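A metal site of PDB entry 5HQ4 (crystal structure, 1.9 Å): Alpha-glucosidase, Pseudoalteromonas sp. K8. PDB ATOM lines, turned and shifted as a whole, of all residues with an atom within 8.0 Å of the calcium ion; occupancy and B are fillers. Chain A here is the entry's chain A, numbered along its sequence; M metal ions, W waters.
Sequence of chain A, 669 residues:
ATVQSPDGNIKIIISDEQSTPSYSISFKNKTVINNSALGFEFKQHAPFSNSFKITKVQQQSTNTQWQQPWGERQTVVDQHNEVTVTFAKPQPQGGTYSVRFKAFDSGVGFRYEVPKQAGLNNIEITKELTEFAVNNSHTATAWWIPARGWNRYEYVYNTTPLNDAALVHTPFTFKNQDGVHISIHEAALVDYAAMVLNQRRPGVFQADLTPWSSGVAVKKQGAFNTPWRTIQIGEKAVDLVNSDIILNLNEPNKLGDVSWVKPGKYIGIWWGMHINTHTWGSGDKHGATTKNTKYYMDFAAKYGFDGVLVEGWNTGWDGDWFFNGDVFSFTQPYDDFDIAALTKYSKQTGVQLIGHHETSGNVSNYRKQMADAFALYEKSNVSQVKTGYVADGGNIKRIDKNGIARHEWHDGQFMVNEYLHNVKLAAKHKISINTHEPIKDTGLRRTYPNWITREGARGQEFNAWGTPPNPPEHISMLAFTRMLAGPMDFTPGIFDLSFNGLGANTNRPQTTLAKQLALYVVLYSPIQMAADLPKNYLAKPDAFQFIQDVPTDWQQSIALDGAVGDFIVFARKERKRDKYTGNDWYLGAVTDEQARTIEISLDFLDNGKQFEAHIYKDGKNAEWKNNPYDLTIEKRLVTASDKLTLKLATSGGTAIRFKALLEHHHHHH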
ATOM      1  N   ASN A 151     -12.702  15.399 -25.313  1.00  0.00           N
ATOM      2  CA  ASN A 151     -11.912  14.171 -25.271  1.00  0.00           C
ATOM      3  C   ASN A 151     -12.317  13.131 -26.322  1.00  0.00           C
ATOM      4  O   ASN A 151     -12.046  11.946 -26.129  1.00  0.00           O
ATOM      5  CB  ASN A 151     -11.939  13.543 -23.882  1.00  0.00           C
ATOM      6  CG  ASN A 151     -10.588  12.993 -23.480  1.00  0.00           C
ATOM      7  OD1 ASN A 151      -9.576  13.576 -23.846  1.00  0.00           O
ATOM      8  ND2 ASN A 151     -10.561  11.867 -22.776  1.00  0.00           N
ATOM      9  N   ARG A 152     -12.943  13.547 -27.435  1.00  0.00           N
ATOM     10  CA  ARG A 152     -13.120  12.679 -28.620  1.00  0.00           C
ATOM     11  C   ARG A 152     -13.995  11.485 -28.252  1.00  0.00           C
ATOM     12  O   ARG A 152     -15.112  11.678 -27.731  1.00  0.00           O
ATOM     13  CB  ARG A 152     -11.748  12.292 -29.193  1.00  0.00           C
ATOM     14  CG  ARG A 152     -10.829  13.462 -29.570  1.00  0.00           C
ATOM     15  CD  ARG A 152      -9.391  12.970 -29.849  1.00  0.00           C
ATOM     16  NE  ARG A 152      -8.964  12.053 -28.803  1.00  0.00           N
ATOM     17  CZ  ARG A 152      -8.461  12.425 -27.628  1.00  0.00           C
ATOM     18  NH1 ARG A 152      -8.286  13.714 -27.341  1.00  0.00           N
ATOM     19  NH2 ARG A 152      -8.131  11.509 -26.740  1.00  0.00           N
ATOM     20  N   GLU A 154     -13.046   9.189 -26.045  1.00  0.00           N
ATOM     21  CA  GLU A 154     -12.502   8.620 -24.811  1.00  0.00           C
ATOM     22  C   GLU A 154     -13.290   9.141 -23.606  1.00  0.00           C
ATOM     23  O   GLU A 154     -12.852   9.988 -22.818  1.00  0.00           O
ATOM     24  CB  GLU A 154     -11.003   8.922 -24.713  1.00  0.00           C
ATOM     25  CG  GLU A 154     -10.172   8.111 -25.739  1.00  0.00           C
ATOM     26  CD  GLU A 154      -8.678   8.454 -25.704  1.00  0.00           C
ATOM     27  OE1 GLU A 154      -7.871   7.602 -26.125  1.00  0.00           O
ATOM     28  OE2 GLU A 154      -8.321   9.555 -25.238  1.00  0.00           O
ATOM     29  N   TRP A 270       6.121   1.110 -22.796  1.00  0.00           N
ATOM     30  CA  TRP A 270       4.854   1.815 -22.949  1.00  0.00           C
ATOM     31  C   TRP A 270       4.238   2.080 -21.577  1.00  0.00           C
ATOM     32  O   TRP A 270       4.138   3.247 -21.160  1.00  0.00           O
ATOM     33  CB  TRP A 270       3.888   0.999 -23.836  1.00  0.00           C
ATOM     34  CG  TRP A 270       2.539   1.662 -23.932  1.00  0.00           C
ATOM     35  CD1 TRP A 270       2.243   2.792 -24.641  1.00  0.00           C
ATOM     36  CD2 TRP A 270       1.340   1.258 -23.279  1.00  0.00           C
ATOM     37  NE1 TRP A 270       0.911   3.116 -24.474  1.00  0.00           N
ATOM     38  CE2 TRP A 270       0.340   2.198 -23.638  1.00  0.00           C
ATOM     39  CE3 TRP A 270       0.999   0.200 -22.421  1.00  0.00           C
ATOM     40  CZ2 TRP A 270      -0.981   2.099 -23.170  1.00  0.00           C
ATOM     41  CZ3 TRP A 270      -0.310   0.107 -21.958  1.00  0.00           C
ATOM     42  CH2 TRP A 270      -1.283   1.051 -22.329  1.00  0.00           C
ATOM     43  N   HIS A 274       3.399   5.456 -18.742  1.00  0.00           N
ATOM     44  CA  HIS A 274       2.100   5.827 -18.198  1.00  0.00           C
ATOM     45  C   HIS A 274       2.064   5.771 -16.672  1.00  0.00           C
ATOM     46  O   HIS A 274       1.324   6.538 -16.050  1.00  0.00           O
ATOM     47  CB  HIS A 274       1.001   4.939 -18.794  1.00  0.00           C
ATOM     48  CG  HIS A 274       0.649   5.313 -20.194  1.00  0.00           C
ATOM     49  ND1 HIS A 274      -0.217   6.334 -20.496  1.00  0.00           N
ATOM     50  CD2 HIS A 274       1.102   4.841 -21.382  1.00  0.00           C
ATOM     51  CE1 HIS A 274      -0.317   6.455 -21.805  1.00  0.00           C
ATOM     52  NE2 HIS A 274       0.476   5.554 -22.368  1.00  0.00           N
ATOM     53  N   TRP A 321       5.014  16.568 -24.274  1.00  0.00           N
ATOM     54  CA  TRP A 321       4.850  16.123 -25.661  1.00  0.00           C
ATOM     55  C   TRP A 321       3.470  16.439 -26.214  1.00  0.00           C
ATOM     56  O   TRP A 321       3.330  16.513 -27.432  1.00  0.00           O
ATOM     57  CB  TRP A 321       5.163  14.616 -25.776  1.00  0.00           C
ATOM     58  CG  TRP A 321       4.309  13.688 -24.956  1.00  0.00           C
ATOM     59  CD1 TRP A 321       4.620  13.142 -23.741  1.00  0.00           C
ATOM     60  CD2 TRP A 321       3.019  13.147 -25.304  1.00  0.00           C
ATOM     61  NE1 TRP A 321       3.612  12.302 -23.309  1.00  0.00           N
ATOM     62  CE2 TRP A 321       2.617  12.296 -24.255  1.00  0.00           C
ATOM     63  CE3 TRP A 321       2.165  13.310 -26.413  1.00  0.00           C
ATOM     64  CZ2 TRP A 321       1.402  11.617 -24.263  1.00  0.00           C
ATOM     65  CZ3 TRP A 321       0.950  12.632 -26.421  1.00  0.00           C
ATOM     66  CH2 TRP A 321       0.584  11.789 -25.357  1.00  0.00           C
ATOM     67  N   GLU A 358       3.410   9.152 -33.147  1.00  0.00           N
ATOM     68  CA  GLU A 358       2.514  10.074 -32.469  1.00  0.00           C
ATOM     69  C   GLU A 358       2.636  11.449 -33.124  1.00  0.00           C
ATOM     70  O   GLU A 358       3.740  11.945 -33.317  1.00  0.00           O
ATOM     71  CB  GLU A 358       2.846  10.168 -30.973  1.00  0.00           C
ATOM     72  CG  GLU A 358       2.034  11.224 -30.183  1.00  0.00           C
ATOM     73  CD  GLU A 358       0.525  10.984 -30.244  1.00  0.00           C
ATOM     74  OE1 GLU A 358      -0.208  11.838 -30.797  1.00  0.00           O
ATOM     75  OE2 GLU A 358       0.060   9.957 -29.733  1.00  0.00           O
ATOM     76  N   LYS A 386       1.888   1.713 -34.705  1.00  0.00           N
ATOM     77  CA  LYS A 386       0.847   2.358 -33.915  1.00  0.00           C
ATOM     78  C   LYS A 386       0.932   3.866 -34.164  1.00  0.00           C
ATOM     79  O   LYS A 386       2.000   4.456 -34.003  1.00  0.00           O
ATOM     80  CB  LYS A 386       1.026   2.032 -32.434  1.00  0.00           C
ATOM     81  CG  LYS A 386       0.120   2.797 -31.465  1.00  0.00           C
ATOM     82  CD  LYS A 386       0.470   2.408 -30.026  1.00  0.00           C
ATOM     83  CE  LYS A 386      -0.225   3.354 -29.031  1.00  0.00           C
ATOM     84  NZ  LYS A 386       0.045   2.990 -27.630  1.00  0.00           N
ATOM     85  N   THR A 387      -0.165   4.466 -34.609  1.00  0.00           N
ATOM     86  CA  THR A 387      -0.199   5.900 -34.851  1.00  0.00           C
ATOM     87  C   THR A 387      -1.006   6.571 -33.744  1.00  0.00           C
ATOM     88  O   THR A 387      -1.709   5.924 -32.973  1.00  0.00           O
ATOM     89  CB  THR A 387      -0.799   6.232 -36.224  1.00  0.00           C
ATOM     90  OG1 THR A 387      -2.141   5.710 -36.316  1.00  0.00           O
ATOM     91  CG2 THR A 387       0.058   5.628 -37.331  1.00  0.00           C
ATOM     92  N   GLY A 388      -0.875   7.897 -33.660  1.00  0.00           N
ATOM     93  CA  GLY A 388      -1.508   8.636 -32.580  1.00  0.00           C
ATOM     94  C   GLY A 388      -1.808  10.053 -32.996  1.00  0.00           C
ATOM     95  O   GLY A 388      -1.053  10.660 -33.756  1.00  0.00           O
ATOM     96  N   TYR A 389      -2.915  10.589 -32.474  1.00  0.00           N
ATOM     97  CA  TYR A 389      -3.373  11.925 -32.842  1.00  0.00           C
ATOM     98  C   TYR A 389      -3.882  12.650 -31.601  1.00  0.00           C
ATOM     99  O   TYR A 389      -5.018  13.121 -31.532  1.00  0.00           O
ATOM    100  CB  TYR A 389      -4.468  11.843 -33.924  1.00  0.00           C
ATOM    101  CG  TYR A 389      -4.015  11.158 -35.187  1.00  0.00           C
ATOM    102  CD1 TYR A 389      -3.951   9.762 -35.263  1.00  0.00           C
ATOM    103  CD2 TYR A 389      -3.608  11.887 -36.302  1.00  0.00           C
ATOM    104  CE1 TYR A 389      -3.509   9.123 -36.405  1.00  0.00           C
ATOM    105  CE2 TYR A 389      -3.168  11.241 -37.460  1.00  0.00           C
ATOM    106  CZ  TYR A 389      -3.123   9.860 -37.501  1.00  0.00           C
ATOM    107  OH  TYR A 389      -2.692   9.201 -38.632  1.00  0.00           O
ATOM    108  N   VAL A 390      -3.027  12.753 -30.575  1.00  0.00           N
ATOM    109  CA  VAL A 390      -3.460  13.280 -29.287  1.00  0.00           C
ATOM    110  C   VAL A 390      -3.631  14.795 -29.397  1.00  0.00           C
ATOM    111  O   VAL A 390      -2.658  15.537 -29.541  1.00  0.00           O
ATOM    112  CB  VAL A 390      -2.481  12.915 -28.162  1.00  0.00           C
ATOM    113  CG1 VAL A 390      -2.886  13.606 -26.857  1.00  0.00           C
ATOM    114  CG2 VAL A 390      -2.442  11.407 -27.964  1.00  0.00           C
ATOM    115  N   THR A 435      -4.470   2.437 -35.098  1.00  0.00           N
ATOM    116  CA  THR A 435      -4.695   3.882 -34.994  1.00  0.00           C
ATOM    117  C   THR A 435      -5.260   4.246 -33.618  1.00  0.00           C
ATOM    118  O   THR A 435      -6.375   3.845 -33.281  1.00  0.00           O
ATOM    119  CB  THR A 435      -5.682   4.363 -36.068  1.00  0.00           C
ATOM    120  OG1 THR A 435      -5.285   3.876 -37.349  1.00  0.00           O
ATOM    121  CG2 THR A 435      -5.724   5.893 -36.095  1.00  0.00           C
ATOM    122  N   HIS A 436      -4.502   5.014 -32.843  1.00  0.00           N
ATOM    123  CA  HIS A 436      -5.045   5.623 -31.633  1.00  0.00           C
ATOM    124  C   HIS A 436      -5.515   7.037 -31.945  1.00  0.00           C
ATOM    125  O   HIS A 436      -5.042   7.659 -32.893  1.00  0.00           O
ATOM    126  CB  HIS A 436      -4.021   5.577 -30.494  1.00  0.00           C
ATOM    127  CG  HIS A 436      -3.876   4.198 -29.904  1.00  0.00           C
ATOM    128  ND1 HIS A 436      -3.811   3.957 -28.547  1.00  0.00           N
ATOM    129  CD2 HIS A 436      -3.850   2.983 -30.506  1.00  0.00           C
ATOM    130  CE1 HIS A 436      -3.728   2.656 -28.342  1.00  0.00           C
ATOM    131  NE2 HIS A 436      -3.753   2.038 -29.511  1.00  0.00           N
ATOM    132  N   GLU A 437      -6.476   7.513 -31.162  1.00  0.00           N
ATOM    133  CA  GLU A 437      -7.255   8.714 -31.489  1.00  0.00           C
ATOM    134  C   GLU A 437      -7.712   8.646 -32.945  1.00  0.00           C
ATOM    135  O   GLU A 437      -7.361   9.500 -33.756  1.00  0.00           O
ATOM    136  CB  GLU A 437      -6.466   9.986 -31.206  1.00  0.00           C
ATOM    137  CG  GLU A 437      -6.019  10.081 -29.741  1.00  0.00           C
ATOM    138  CD  GLU A 437      -4.844   9.148 -29.425  1.00  0.00           C
ATOM    139  OE1 GLU A 437      -3.884   9.130 -30.225  1.00  0.00           O
ATOM    140  OE2 GLU A 437      -4.885   8.415 -28.422  1.00  0.00           O
ATOM    141  N   PRO A 438      -8.490   7.629 -33.302  1.00  0.00           N
ATOM    142  CA  PRO A 438      -8.821   7.369 -34.702  1.00  0.00           C
ATOM    143  C   PRO A 438     -10.151   7.973 -35.106  1.00  0.00           C
ATOM    144  O   PRO A 438     -10.828   8.586 -34.282  1.00  0.00           O
ATOM    145  CB  PRO A 438      -8.935   5.837 -34.727  1.00  0.00           C
ATOM    146  CG  PRO A 438      -9.694   5.584 -33.435  1.00  0.00           C
ATOM    147  CD  PRO A 438      -9.100   6.612 -32.420  1.00  0.00           C
ATOM    148  N   GLU A 455      -7.965   2.356 -31.339  1.00  0.00           N
ATOM    149  CA  GLU A 455      -8.444   2.605 -29.988  1.00  0.00           C
ATOM    150  C   GLU A 455      -9.836   3.235 -30.067  1.00  0.00           C
ATOM    151  O   GLU A 455     -10.820   2.513 -30.238  1.00  0.00           O
ATOM    152  CB  GLU A 455      -7.437   3.495 -29.236  1.00  0.00           C
ATOM    153  CG  GLU A 455      -7.668   3.597 -27.747  1.00  0.00           C
ATOM    154  CD  GLU A 455      -6.546   4.370 -27.082  1.00  0.00           C
ATOM    155  OE1 GLU A 455      -6.357   5.553 -27.448  1.00  0.00           O
ATOM    156  OE2 GLU A 455      -5.826   3.800 -26.239  1.00  0.00           O
ATOM    157  N   GLY A 456      -9.938   4.562 -29.966  1.00  0.00           N
ATOM    158  CA  GLY A 456     -11.259   5.171 -30.169  1.00  0.00           C
ATOM    159  C   GLY A 456     -12.257   4.871 -29.070  1.00  0.00           C
ATOM    160  O   GLY A 456     -13.461   4.707 -29.353  1.00  0.00           O
ATOM    161  N   ALA A 457     -11.795   4.820 -27.829  1.00  0.00           N
ATOM    162  CA  ALA A 457     -12.542   4.531 -26.619  1.00  0.00           C
ATOM    163  C   ALA A 457     -11.513   4.552 -25.505  1.00  0.00           C
ATOM    164  O   ALA A 457     -10.310   4.502 -25.771  1.00  0.00           O
ATOM    165  CB  ALA A 457     -13.251   3.172 -26.675  1.00  0.00           C
ATOM    166  N   ARG A 458     -11.979   4.638 -24.260  1.00  0.00           N
ATOM    167  CA  ARG A 458     -11.044   4.572 -23.137  1.00  0.00           C
ATOM    168  C   ARG A 458     -10.547   3.140 -22.975  1.00  0.00           C
ATOM    169  O   ARG A 458     -11.334   2.218 -22.738  1.00  0.00           O
ATOM    170  CB  ARG A 458     -11.703   5.049 -21.843  1.00  0.00           C
ATOM    171  CG  ARG A 458     -11.897   6.577 -21.782  1.00  0.00           C
ATOM    172  CD  ARG A 458     -12.676   6.999 -20.540  1.00  0.00           C
ATOM    173  NE  ARG A 458     -12.111   6.475 -19.278  1.00  0.00           N
ATOM    174  CZ  ARG A 458     -11.801   7.225 -18.220  1.00  0.00           C
ATOM    175  NH1 ARG A 458     -11.988   8.537 -18.246  1.00  0.00           N
ATOM    176  NH2 ARG A 458     -11.345   6.650 -17.110  1.00  0.00           N
ATOM    177  N   GLY A 459      -9.238   2.960 -23.127  1.00  0.00           N
ATOM    178  CA  GLY A 459      -8.595   1.681 -22.904  1.00  0.00           C
ATOM    179  C   GLY A 459      -7.875   1.649 -21.570  1.00  0.00           C
ATOM    180  O   GLY A 459      -8.119   2.475 -20.680  1.00  0.00           O
ATOM    181  N   GLU A 461      -4.977   2.571 -20.684  1.00  0.00           N
ATOM    182  CA  GLU A 461      -4.137   3.696 -20.303  1.00  0.00           C
ATOM    183  C   GLU A 461      -4.848   4.624 -19.310  1.00  0.00           C
ATOM    184  O   GLU A 461      -4.206   5.214 -18.448  1.00  0.00           O
ATOM    185  CB  GLU A 461      -3.690   4.481 -21.540  1.00  0.00           C
ATOM    186  CG  GLU A 461      -4.883   5.025 -22.342  1.00  0.00           C
ATOM    187  CD  GLU A 461      -4.482   5.951 -23.482  1.00  0.00           C
ATOM    188  OE1 GLU A 461      -3.301   6.372 -23.524  1.00  0.00           O
ATOM    189  OE2 GLU A 461      -5.357   6.255 -24.326  1.00  0.00           O
ATOM    190  N   PHE A 462      -6.175   4.731 -19.403  1.00  0.00           N
ATOM    191  CA  PHE A 462      -6.910   5.561 -18.452  1.00  0.00           C
ATOM    192  C   PHE A 462      -6.921   4.978 -17.048  1.00  0.00           C
ATOM    193  O   PHE A 462      -7.294   5.689 -16.104  1.00  0.00           O
ATOM    194  CB  PHE A 462      -8.353   5.782 -18.932  1.00  0.00           C
ATOM    195  CG  PHE A 462      -8.463   6.831 -19.986  1.00  0.00           C
ATOM    196  CD1 PHE A 462      -8.142   6.531 -21.309  1.00  0.00           C
ATOM    197  CD2 PHE A 462      -8.810   8.139 -19.653  1.00  0.00           C
ATOM    198  CE1 PHE A 462      -8.200   7.522 -22.293  1.00  0.00           C
ATOM    199  CE2 PHE A 462      -8.871   9.126 -20.628  1.00  0.00           C
ATOM    200  CZ  PHE A 462      -8.561   8.806 -21.940  1.00  0.00           C
ATOM    201  N   TRP A 465      -3.913   6.823 -14.985  1.00  0.00           N
ATOM    202  CA  TRP A 465      -3.983   8.207 -14.538  1.00  0.00           C
ATOM    203  C   TRP A 465      -5.357   8.842 -14.712  1.00  0.00           C
ATOM    204  O   TRP A 465      -5.464  10.069 -14.590  1.00  0.00           O
ATOM    205  CB  TRP A 465      -2.933   9.047 -15.290  1.00  0.00           C
ATOM    206  CG  TRP A 465      -2.792   8.610 -16.734  1.00  0.00           C
ATOM    207  CD1 TRP A 465      -1.755   7.905 -17.277  1.00  0.00           C
ATOM    208  CD2 TRP A 465      -3.734   8.824 -17.802  1.00  0.00           C
ATOM    209  NE1 TRP A 465      -1.993   7.662 -18.616  1.00  0.00           N
ATOM    210  CE2 TRP A 465      -3.192   8.222 -18.963  1.00  0.00           C
ATOM    211  CE3 TRP A 465      -4.971   9.475 -17.890  1.00  0.00           C
ATOM    212  CZ2 TRP A 465      -3.847   8.238 -20.203  1.00  0.00           C
ATOM    213  CZ3 TRP A 465      -5.630   9.500 -19.127  1.00  0.00           C
ATOM    214  CH2 TRP A 465      -5.059   8.879 -20.264  1.00  0.00           C
HETATM  215 CA    CA M   1      -5.395   7.428 -26.345  1.00  0.00          CA
HETATM  216  O   HOH W   1      -3.301   9.035 -24.770  1.00  0.00           O
HETATM  217  O   HOH W   2      -3.465   6.177 -27.001  1.00  0.00           O
HETATM  218  O   HOH W   3      -5.629   9.571 -25.322  1.00  0.00           O
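The calcium ion is bound by OE2 of Glu 461, OE2 of Glu 437, OE1 of Glu 455, water W3, water W2 and OE1 of Glu 154.
Slightly farther from the calcium ion lies water W1 (3.1 Å).
Of the 24 residues printed, 4 come within 4 Å of the calcium ion.
The nearest printed residue that does not touch the calcium ion is His 436 (4.4 Å).
The indole nitrogen (NE1) of Trp 465 lies close to the backbone carbonyl oxygen (O) of Glu 461, at 3.3 Å.
OE1 of Glu 437 is in hydrogen-bond range of N of Tyr 389 (2.9 Å).
A ring nitrogen (ND1) of His 436 sits at hydrogen-bond distance from the side-chain carboxylate (OE2) of Glu 455 (3.1 Å).
The backbone NH of Glu 455 sits at hydrogen-bond distance from the backbone carbonyl oxygen of Thr 435, 2.9 Å away.
The side-chain carboxylate of Glu 154 is in salt-bridge range of the guanidinium group of Arg 152 (2.5 Å).
ND2 of Asn 151 sits at hydrogen-bond distance from O of Glu 154 (3.0 Å).
Water W3 lies within hydrogen-bond range of the side-chain carboxylate of Glu 154 and the guanidinium group of Arg 152.
Water W2 lies within hydrogen-bond range of a ring nitrogen (ND1) of His 436 (2.7 Å), the side-chain carboxylate (OE2) of Glu 455 (3.4 Å) and the side-chain carboxylate (OE1) of Glu 461 (3.5 Å).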
